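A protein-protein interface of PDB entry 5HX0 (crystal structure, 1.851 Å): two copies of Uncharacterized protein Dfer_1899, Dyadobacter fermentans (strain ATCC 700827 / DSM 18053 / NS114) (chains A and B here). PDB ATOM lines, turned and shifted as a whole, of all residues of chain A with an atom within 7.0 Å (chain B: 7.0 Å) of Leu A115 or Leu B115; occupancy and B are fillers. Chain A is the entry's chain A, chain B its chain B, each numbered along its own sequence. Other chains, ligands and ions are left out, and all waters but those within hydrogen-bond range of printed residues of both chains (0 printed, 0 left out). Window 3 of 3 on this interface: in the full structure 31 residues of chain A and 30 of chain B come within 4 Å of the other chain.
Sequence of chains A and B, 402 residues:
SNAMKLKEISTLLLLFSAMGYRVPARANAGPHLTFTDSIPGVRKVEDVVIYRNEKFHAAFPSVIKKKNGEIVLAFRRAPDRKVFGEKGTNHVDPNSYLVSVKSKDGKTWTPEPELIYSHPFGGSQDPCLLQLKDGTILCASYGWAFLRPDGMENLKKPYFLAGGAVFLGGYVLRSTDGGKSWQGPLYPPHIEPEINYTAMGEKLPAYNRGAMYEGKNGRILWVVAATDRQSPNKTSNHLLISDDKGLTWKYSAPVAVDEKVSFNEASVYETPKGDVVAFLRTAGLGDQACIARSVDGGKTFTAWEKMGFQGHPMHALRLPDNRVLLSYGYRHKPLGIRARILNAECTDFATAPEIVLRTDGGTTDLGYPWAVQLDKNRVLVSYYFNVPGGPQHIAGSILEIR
The side-chain hydroxyl of Ser A118 lies within hydrogen-bond range of the side-chain hydroxyl of Ser B118 (2.8 Å).
Among the printed residues, merely in contact across the chains: Leu A115 with Leu B115 (3.3 Å), Ser A118 with Tyr B97 (3.5 Å), Tyr A97 with Ser B118 (3.5 Å), Tyr A97 with Tyr B97 (3.6 Å), Lys A180 with Lys B180 (3.8 Å) and Ser A118 with Leu B115 (3.9 Å).
Glu A112 touches none of the printed residues of chain B. Printed residues of chain B within 4 Å of Leu A115: Leu B115 (3.3 Å). Of the printed residues of chain B, Ser A118 touches Tyr B97 (3.5 Å), Leu B115 (3.9 Å) and Ser B118 (2.8 Å). Printed residues of chain B within 4 Å of Lys A180: Lys B180 (3.8 Å). Printed residues of chain A within 4 Å of Tyr B97: Tyr A97 (3.6 Å) and Ser A118 (3.5 Å). Printed residues of chain A within 4 Å of Leu B115: Leu A115 and Ser A118. The nearest printed residue of chain A that does not touch Leu B115 is Tyr A117 (6.6 Å). The nearest printed residue of chain A that does not touch Ser B118 is Leu A115 (4.6 Å).
Printed residues of chain A that touch a printed residue of chain B: Tyr A97, Leu A115, Ser A118 and Lys A180. Hydrophobic or aromatic side chains of chain A that line the printed part of chain B: Tyr A97 and Leu A115. Of the 14 printed residues of chain B, 4 touch a printed residue of chain A. Hydrophobic or aromatic side chains of chain B that line the printed part of chain A: Tyr B97 and Leu B115. Along chain B the printed residues that touch a printed residue of chain A span positions 97 to 180. Among the printed residues, no Asp or Glu carboxylate lies within 4 Å of a Lys or Arg side-chain nitrogen of the other chain.
Tyr A97 touches Ser B118, and with the chains exchanged Ser A118 touches Tyr B97. Leu B115 touches its own counterpart, Leu A115. Ser A118 touches Leu B115, but with the chains exchanged Leu A115 does not touch Ser B118 (4.6 Å). Lys A180 touches its own counterpart, Lys B180. Positions printed for both chains: 97, 98, 99, 100, 112, 113, 114, 115, 116, 117, 118, 179, 180 and 182.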
ATOM      1  N   TYR A  97       1.335   6.121  14.682  1.00  0.00           N
ATOM      2  CA  TYR A  97       0.695   7.423  14.759  1.00  0.00           C
ATOM      3  C   TYR A  97       0.525   8.031  13.375  1.00  0.00           C
ATOM      4  O   TYR A  97       1.209   7.669  12.421  1.00  0.00           O
ATOM      5  CB  TYR A  97       1.513   8.396  15.619  1.00  0.00           C
ATOM      6  CG  TYR A  97       1.816   7.899  17.024  1.00  0.00           C
ATOM      7  CD1 TYR A  97       0.946   7.046  17.689  1.00  0.00           C
ATOM      8  CD2 TYR A  97       2.981   8.292  17.676  1.00  0.00           C
ATOM      9  CE1 TYR A  97       1.221   6.594  18.997  1.00  0.00           C
ATOM     10  CE2 TYR A  97       3.274   7.854  18.972  1.00  0.00           C
ATOM     11  CZ  TYR A  97       2.402   7.011  19.632  1.00  0.00           C
ATOM     12  OH  TYR A  97       2.722   6.585  20.922  1.00  0.00           O
ATOM     13  N   LEU A  98      -0.389   8.984  13.282  1.00  0.00           N
ATOM     14  CA  LEU A  98      -0.564   9.767  12.064  1.00  0.00           C
ATOM     15  C   LEU A  98       0.300  11.017  12.187  1.00  0.00           C
ATOM     16  O   LEU A  98       0.109  11.815  13.113  1.00  0.00           O
ATOM     17  CB  LEU A  98      -2.037  10.122  11.869  1.00  0.00           C
ATOM     18  CG  LEU A  98      -3.069   8.973  11.948  1.00  0.00           C
ATOM     19  CD1 LEU A  98      -4.478   9.482  11.555  1.00  0.00           C
ATOM     20  CD2 LEU A  98      -2.683   7.760  11.087  1.00  0.00           C
ATOM     21  N   VAL A  99       1.259  11.184  11.270  1.00  0.00           N
ATOM     22  CA  VAL A  99       2.191  12.309  11.323  1.00  0.00           C
ATOM     23  C   VAL A  99       2.256  12.977   9.954  1.00  0.00           C
ATOM     24  O   VAL A  99       1.741  12.463   8.959  1.00  0.00           O
ATOM     25  CB  VAL A  99       3.604  11.868  11.783  1.00  0.00           C
ATOM     26  CG1 VAL A  99       3.546  11.203  13.164  1.00  0.00           C
ATOM     27  CG2 VAL A  99       4.223  10.934  10.790  1.00  0.00           C
ATOM     28  N   SER A 100       2.930  14.129   9.900  1.00  0.00           N
ATOM     29  CA  SER A 100       3.058  14.859   8.643  1.00  0.00           C
ATOM     30  C   SER A 100       4.435  15.490   8.499  1.00  0.00           C
ATOM     31  O   SER A 100       5.099  15.811   9.491  1.00  0.00           O
ATOM     32  CB  SER A 100       2.002  15.980   8.520  1.00  0.00           C
ATOM     33  OG  SER A 100       2.240  16.962   9.514  1.00  0.00           O
ATOM     34  N   GLU A 112      11.522  16.899  10.750  1.00  0.00           N
ATOM     35  CA  GLU A 112      10.909  16.287  11.931  1.00  0.00           C
ATOM     36  C   GLU A 112       9.392  16.227  11.768  1.00  0.00           C
ATOM     37  O   GLU A 112       8.747  17.285  11.727  1.00  0.00           O
ATOM     38  CB  GLU A 112      11.271  17.085  13.190  1.00  0.00           C
ATOM     39  CG  GLU A 112      10.861  16.408  14.473  1.00  0.00           C
ATOM     40  CD  GLU A 112      11.688  15.157  14.748  1.00  0.00           C
ATOM     41  OE1 GLU A 112      12.828  15.052  14.226  1.00  0.00           O
ATOM     42  OE2 GLU A 112      11.195  14.277  15.485  1.00  0.00           O
ATOM     43  N   PRO A 113       8.781  15.043  11.669  1.00  0.00           N
ATOM     44  CA  PRO A 113       7.333  14.975  11.462  1.00  0.00           C
ATOM     45  C   PRO A 113       6.556  15.565  12.626  1.00  0.00           C
ATOM     46  O   PRO A 113       6.928  15.394  13.789  1.00  0.00           O
ATOM     47  CB  PRO A 113       7.066  13.477  11.323  1.00  0.00           C
ATOM     48  CG  PRO A 113       8.399  12.910  10.823  1.00  0.00           C
ATOM     49  CD  PRO A 113       9.418  13.715  11.558  1.00  0.00           C
ATOM     50  N   GLU A 114       5.481  16.281  12.307  1.00  0.00           N
ATOM     51  CA  GLU A 114       4.551  16.745  13.336  1.00  0.00           C
ATOM     52  C   GLU A 114       3.445  15.719  13.534  1.00  0.00           C
ATOM     53  O   GLU A 114       3.051  15.024  12.601  1.00  0.00           O
ATOM     54  CB  GLU A 114       3.920  18.081  12.952  1.00  0.00           C
ATOM     55  CG  GLU A 114       4.890  19.227  12.921  1.00  0.00           C
ATOM     56  CD  GLU A 114       4.199  20.496  12.514  1.00  0.00           C
ATOM     57  OE1 GLU A 114       3.962  20.697  11.301  1.00  0.00           O
ATOM     58  OE2 GLU A 114       3.856  21.273  13.423  1.00  0.00           O
ATOM     59  N   LEU A 115       2.914  15.659  14.749  1.00  0.00           N
ATOM     60  CA  LEU A 115       1.853  14.708  15.043  1.00  0.00           C
ATOM     61  C   LEU A 115       0.507  15.257  14.588  1.00  0.00           C
ATOM     62  O   LEU A 115       0.132  16.382  14.935  1.00  0.00           O
ATOM     63  CB  LEU A 115       1.807  14.398  16.537  1.00  0.00           C
ATOM     64  CG  LEU A 115       0.738  13.352  16.862  1.00  0.00           C
ATOM     65  CD1 LEU A 115       1.204  11.968  16.527  1.00  0.00           C
ATOM     66  CD2 LEU A 115       0.383  13.420  18.300  1.00  0.00           C
ATOM     67  N   ILE A 116      -0.196  14.476  13.778  1.00  0.00           N
ATOM     68  CA  ILE A 116      -1.608  14.732  13.512  1.00  0.00           C
ATOM     69  C   ILE A 116      -2.479  14.054  14.561  1.00  0.00           C
ATOM     70  O   ILE A 116      -3.377  14.671  15.137  1.00  0.00           O
ATOM     71  CB  ILE A 116      -1.999  14.268  12.090  1.00  0.00           C
ATOM     72  CG1 ILE A 116      -1.313  15.123  11.023  1.00  0.00           C
ATOM     73  CG2 ILE A 116      -3.537  14.333  11.922  1.00  0.00           C
ATOM     74  CD1 ILE A 116      -1.470  14.548   9.575  1.00  0.00           C
ATOM     75  N   TYR A 117      -2.211  12.785  14.853  1.00  0.00           N
ATOM     76  CA  TYR A 117      -3.093  12.071  15.766  1.00  0.00           C
ATOM     77  C   TYR A 117      -2.455  10.807  16.314  1.00  0.00           C
ATOM     78  O   TYR A 117      -1.861  10.025  15.562  1.00  0.00           O
ATOM     79  CB  TYR A 117      -4.386  11.701  15.057  1.00  0.00           C
ATOM     80  CG  TYR A 117      -5.430  11.086  15.971  1.00  0.00           C
ATOM     81  CD1 TYR A 117      -6.017  11.829  16.992  1.00  0.00           C
ATOM     82  CD2 TYR A 117      -5.858   9.776  15.773  1.00  0.00           C
ATOM     83  CE1 TYR A 117      -6.990  11.265  17.819  1.00  0.00           C
ATOM     84  CE2 TYR A 117      -6.833   9.202  16.584  1.00  0.00           C
ATOM     85  CZ  TYR A 117      -7.390   9.957  17.608  1.00  0.00           C
ATOM     86  OH  TYR A 117      -8.347   9.384  18.412  1.00  0.00           O
ATOM     87  N   SER A 118      -2.603  10.607  17.622  1.00  0.00           N
ATOM     88  CA  SER A 118      -2.317   9.335  18.277  1.00  0.00           C
ATOM     89  C   SER A 118      -3.590   8.866  18.965  1.00  0.00           C
ATOM     90  O   SER A 118      -4.111   9.551  19.856  1.00  0.00           O
ATOM     91  CB  SER A 118      -1.176   9.468  19.284  1.00  0.00           C
ATOM     92  OG  SER A 118      -1.336  10.627  20.085  1.00  0.00           O
ATOM     93  N   GLY A 179      -4.847  22.684   9.425  1.00  0.00           N
ATOM     94  CA  GLY A 179      -4.007  21.645   9.988  1.00  0.00           C
ATOM     95  C   GLY A 179      -3.219  22.068  11.204  1.00  0.00           C
ATOM     96  O   GLY A 179      -2.372  21.302  11.675  1.00  0.00           O
ATOM     97  N   LYS A 180      -3.467  23.266  11.733  1.00  0.00           N
ATOM     98  CA  LYS A 180      -2.798  23.655  12.967  1.00  0.00           C
ATOM     99  C   LYS A 180      -3.301  22.818  14.137  1.00  0.00           C
ATOM    100  O   LYS A 180      -2.521  22.428  15.016  1.00  0.00           O
ATOM    101  CB  LYS A 180      -3.015  25.143  13.219  1.00  0.00           C
ATOM    102  CG  LYS A 180      -2.121  25.747  14.297  1.00  0.00           C
ATOM    103  CD  LYS A 180      -2.546  27.190  14.587  1.00  0.00           C
ATOM    104  CE  LYS A 180      -1.787  27.809  15.764  1.00  0.00           C
ATOM    105  NZ  LYS A 180      -0.350  28.095  15.462  1.00  0.00           N
ATOM    106  N   TRP A 182      -6.506  19.668  15.206  1.00  0.00           N
ATOM    107  CA  TRP A 182      -7.419  18.657  14.682  1.00  0.00           C
ATOM    108  C   TRP A 182      -8.478  18.375  15.726  1.00  0.00           C
ATOM    109  O   TRP A 182      -8.157  18.173  16.902  1.00  0.00           O
ATOM    110  CB  TRP A 182      -6.650  17.375  14.331  1.00  0.00           C
ATOM    111  CG  TRP A 182      -5.588  17.613  13.312  1.00  0.00           C
ATOM    112  CD1 TRP A 182      -4.283  17.961  13.539  1.00  0.00           C
ATOM    113  CD2 TRP A 182      -5.743  17.546  11.892  1.00  0.00           C
ATOM    114  NE1 TRP A 182      -3.617  18.102  12.346  1.00  0.00           N
ATOM    115  CE2 TRP A 182      -4.490  17.851  11.320  1.00  0.00           C
ATOM    116  CE3 TRP A 182      -6.819  17.247  11.047  1.00  0.00           C
ATOM    117  CZ2 TRP A 182      -4.278  17.867   9.950  1.00  0.00           C
ATOM    118  CZ3 TRP A 182      -6.600  17.262   9.677  1.00  0.00           C
ATOM    119  CH2 TRP A 182      -5.347  17.570   9.148  1.00  0.00           C
ATOM    120  N   TYR B  97      -0.259   8.177  27.227  1.00  0.00           N
ATOM    121  CA  TYR B  97       0.259   9.417  26.674  1.00  0.00           C
ATOM    122  C   TYR B  97       0.356  10.465  27.783  1.00  0.00           C
ATOM    123  O   TYR B  97      -0.326  10.384  28.797  1.00  0.00           O
ATOM    124  CB  TYR B  97      -0.637   9.961  25.548  1.00  0.00           C
ATOM    125  CG  TYR B  97      -0.896   9.007  24.389  1.00  0.00           C
ATOM    126  CD1 TYR B  97       0.051   8.064  23.999  1.00  0.00           C
ATOM    127  CD2 TYR B  97      -2.100   9.062  23.683  1.00  0.00           C
ATOM    128  CE1 TYR B  97      -0.193   7.194  22.928  1.00  0.00           C
ATOM    129  CE2 TYR B  97      -2.346   8.209  22.616  1.00  0.00           C
ATOM    130  CZ  TYR B  97      -1.394   7.275  22.242  1.00  0.00           C
ATOM    131  OH  TYR B  97      -1.660   6.418  21.179  1.00  0.00           O
ATOM    132  N   LEU B  98       1.202  11.456  27.577  1.00  0.00           N
ATOM    133  CA  LEU B  98       1.282  12.593  28.488  1.00  0.00           C
ATOM    134  C   LEU B  98       0.348  13.680  27.963  1.00  0.00           C
ATOM    135  O   LEU B  98       0.493  14.126  26.815  1.00  0.00           O
ATOM    136  CB  LEU B  98       2.720  13.091  28.574  1.00  0.00           C
ATOM    137  CG  LEU B  98       3.811  12.036  28.841  1.00  0.00           C
ATOM    138  CD1 LEU B  98       5.166  12.735  28.963  1.00  0.00           C
ATOM    139  CD2 LEU B  98       3.520  11.189  30.080  1.00  0.00           C
ATOM    140  N   VAL B  99      -0.624  14.085  28.781  1.00  0.00           N
ATOM    141  CA  VAL B  99      -1.654  15.031  28.374  1.00  0.00           C
ATOM    142  C   VAL B  99      -1.808  16.076  29.470  1.00  0.00           C
ATOM    143  O   VAL B  99      -1.312  15.919  30.588  1.00  0.00           O
ATOM    144  CB  VAL B  99      -3.013  14.342  28.080  1.00  0.00           C
ATOM    145  CG1 VAL B  99      -2.857  13.254  27.004  1.00  0.00           C
ATOM    146  CG2 VAL B  99      -3.609  13.746  29.350  1.00  0.00           C
ATOM    147  N   SER B 100      -2.525  17.154  29.147  1.00  0.00           N
ATOM    148  CA  SER B 100      -2.675  18.245  30.102  1.00  0.00           C
ATOM    149  C   SER B 100      -4.095  18.795  30.095  1.00  0.00           C
ATOM    150  O   SER B 100      -4.799  18.737  29.087  1.00  0.00           O
ATOM    151  CB  SER B 100      -1.710  19.393  29.801  1.00  0.00           C
ATOM    152  OG  SER B 100      -2.054  20.038  28.584  1.00  0.00           O
ATOM    153  N   GLU B 112     -11.301  18.828  27.809  1.00  0.00           N
ATOM    154  CA  GLU B 112     -10.680  17.935  26.838  1.00  0.00           C
ATOM    155  C   GLU B 112      -9.165  18.039  26.928  1.00  0.00           C
ATOM    156  O   GLU B 112      -8.602  19.080  26.546  1.00  0.00           O
ATOM    157  CB  GLU B 112     -11.158  18.283  25.427  1.00  0.00           C
ATOM    158  CG  GLU B 112     -10.427  17.539  24.330  1.00  0.00           C
ATOM    159  CD  GLU B 112     -10.610  16.033  24.426  1.00  0.00           C
ATOM    160  OE1 GLU B 112     -11.674  15.585  24.915  1.00  0.00           O
ATOM    161  OE2 GLU B 112      -9.681  15.303  24.014  1.00  0.00           O
ATOM    162  N   PRO B 113      -8.465  16.999  27.394  1.00  0.00           N
ATOM    163  CA  PRO B 113      -7.006  17.109  27.581  1.00  0.00           C
ATOM    164  C   PRO B 113      -6.265  17.363  26.273  1.00  0.00           C
ATOM    165  O   PRO B 113      -6.581  16.783  25.234  1.00  0.00           O
ATOM    166  CB  PRO B 113      -6.621  15.746  28.177  1.00  0.00           C
ATOM    167  CG  PRO B 113      -7.905  15.213  28.791  1.00  0.00           C
ATOM    168  CD  PRO B 113      -9.008  15.725  27.905  1.00  0.00           C
ATOM    169  N   GLU B 114      -5.264  18.239  26.330  1.00  0.00           N
ATOM    170  CA  GLU B 114      -4.382  18.434  25.185  1.00  0.00           C
ATOM    171  C   GLU B 114      -3.215  17.470  25.291  1.00  0.00           C
ATOM    172  O   GLU B 114      -2.818  17.079  26.384  1.00  0.00           O
ATOM    173  CB  GLU B 114      -3.847  19.861  25.118  1.00  0.00           C
ATOM    174  CG  GLU B 114      -4.914  20.913  24.952  1.00  0.00           C
ATOM    175  CD  GLU B 114      -4.319  22.294  24.766  1.00  0.00           C
ATOM    176  OE1 GLU B 114      -4.008  22.961  25.774  1.00  0.00           O
ATOM    177  OE2 GLU B 114      -4.145  22.699  23.604  1.00  0.00           O
ATOM    178  N   LEU B 115      -2.657  17.095  24.151  1.00  0.00           N
ATOM    179  CA  LEU B 115      -1.554  16.143  24.162  1.00  0.00           C
ATOM    180  C   LEU B 115      -0.249  16.886  24.397  1.00  0.00           C
ATOM    181  O   LEU B 115       0.031  17.887  23.733  1.00  0.00           O
ATOM    182  CB  LEU B 115      -1.495  15.355  22.858  1.00  0.00           C
ATOM    183  CG  LEU B 115      -0.324  14.362  22.876  1.00  0.00           C
ATOM    184  CD1 LEU B 115      -0.667  13.100  23.669  1.00  0.00           C
ATOM    185  CD2 LEU B 115       0.052  14.011  21.505  1.00  0.00           C
ATOM    186  N   ILE B 116       0.528  16.425  25.375  1.00  0.00           N
ATOM    187  CA  ILE B 116       1.915  16.868  25.496  1.00  0.00           C
ATOM    188  C   ILE B 116       2.844  15.982  24.676  1.00  0.00           C
ATOM    189  O   ILE B 116       3.686  16.474  23.906  1.00  0.00           O
ATOM    190  CB  ILE B 116       2.355  16.888  26.979  1.00  0.00           C
ATOM    191  CG1 ILE B 116       1.637  17.992  27.734  1.00  0.00           C
ATOM    192  CG2 ILE B 116       3.862  17.132  27.060  1.00  0.00           C
ATOM    193  CD1 ILE B 116       1.969  18.010  29.213  1.00  0.00           C
ATOM    194  N   TYR B 117       2.708  14.660  24.824  1.00  0.00           N
ATOM    195  CA  TYR B 117       3.640  13.784  24.136  1.00  0.00           C
ATOM    196  C   TYR B 117       3.100  12.367  24.068  1.00  0.00           C
ATOM    197  O   TYR B 117       2.589  11.839  25.064  1.00  0.00           O
ATOM    198  CB  TYR B 117       4.988  13.800  24.855  1.00  0.00           C
ATOM    199  CG  TYR B 117       6.102  12.998  24.202  1.00  0.00           C
ATOM    200  CD1 TYR B 117       6.598  13.349  22.951  1.00  0.00           C
ATOM    201  CD2 TYR B 117       6.679  11.912  24.861  1.00  0.00           C
ATOM    202  CE1 TYR B 117       7.634  12.626  22.361  1.00  0.00           C
ATOM    203  CE2 TYR B 117       7.725  11.193  24.285  1.00  0.00           C
ATOM    204  CZ  TYR B 117       8.193  11.558  23.036  1.00  0.00           C
ATOM    205  OH  TYR B 117       9.215  10.840  22.450  1.00  0.00           O
ATOM    206  N   SER B 118       3.182  11.771  22.878  1.00  0.00           N
ATOM    207  CA  SER B 118       3.069  10.330  22.677  1.00  0.00           C
ATOM    208  C   SER B 118       4.432   9.838  22.212  1.00  0.00           C
ATOM    209  O   SER B 118       4.948  10.309  21.189  1.00  0.00           O
ATOM    210  CB  SER B 118       1.998   9.982  21.640  1.00  0.00           C
ATOM    211  OG  SER B 118       0.756  10.608  21.915  1.00  0.00           O
ATOM    212  N   GLY B 179       4.651  26.028  26.676  1.00  0.00           N
ATOM    213  CA  GLY B 179       3.874  24.810  26.542  1.00  0.00           C
ATOM    214  C   GLY B 179       3.036  24.707  25.288  1.00  0.00           C
ATOM    215  O   GLY B 179       2.218  23.782  25.183  1.00  0.00           O
ATOM    216  N   LYS B 180       3.197  25.640  24.345  1.00  0.00           N
ATOM    217  CA  LYS B 180       2.535  25.518  23.054  1.00  0.00           C
ATOM    218  C   LYS B 180       3.115  24.353  22.261  1.00  0.00           C
ATOM    219  O   LYS B 180       2.374  23.548  21.691  1.00  0.00           O
ATOM    220  CB  LYS B 180       2.679  26.832  22.283  1.00  0.00           C
ATOM    221  CG  LYS B 180       2.054  26.833  20.905  1.00  0.00           C
ATOM    222  CD  LYS B 180       2.426  28.097  20.119  1.00  0.00           C
ATOM    223  CE  LYS B 180       1.920  28.021  18.681  1.00  0.00           C
ATOM    224  NZ  LYS B 180       2.369  29.182  17.868  1.00  0.00           N
ATOM    225  N   TRP B 182       6.584  21.340  22.170  1.00  0.00           N
ATOM    226  CA  TRP B 182       7.555  20.641  22.988  1.00  0.00           C
ATOM    227  C   TRP B 182       8.629  20.088  22.072  1.00  0.00           C
ATOM    228  O   TRP B 182       8.315  19.422  21.085  1.00  0.00           O
ATOM    229  CB  TRP B 182       6.876  19.513  23.772  1.00  0.00           C
ATOM    230  CG  TRP B 182       5.783  19.998  24.687  1.00  0.00           C
ATOM    231  CD1 TRP B 182       4.458  20.140  24.389  1.00  0.00           C
ATOM    232  CD2 TRP B 182       5.928  20.383  26.056  1.00  0.00           C
ATOM    233  NE1 TRP B 182       3.772  20.602  25.475  1.00  0.00           N
ATOM    234  CE2 TRP B 182       4.646  20.765  26.517  1.00  0.00           C
ATOM    235  CE3 TRP B 182       7.022  20.461  26.934  1.00  0.00           C
ATOM    236  CZ2 TRP B 182       4.420  21.214  27.815  1.00  0.00           C
ATOM    237  CZ3 TRP B 182       6.795  20.907  28.235  1.00  0.00           C
ATOM    238  CH2 TRP B 182       5.496  21.268  28.662  1.00  0.00           C
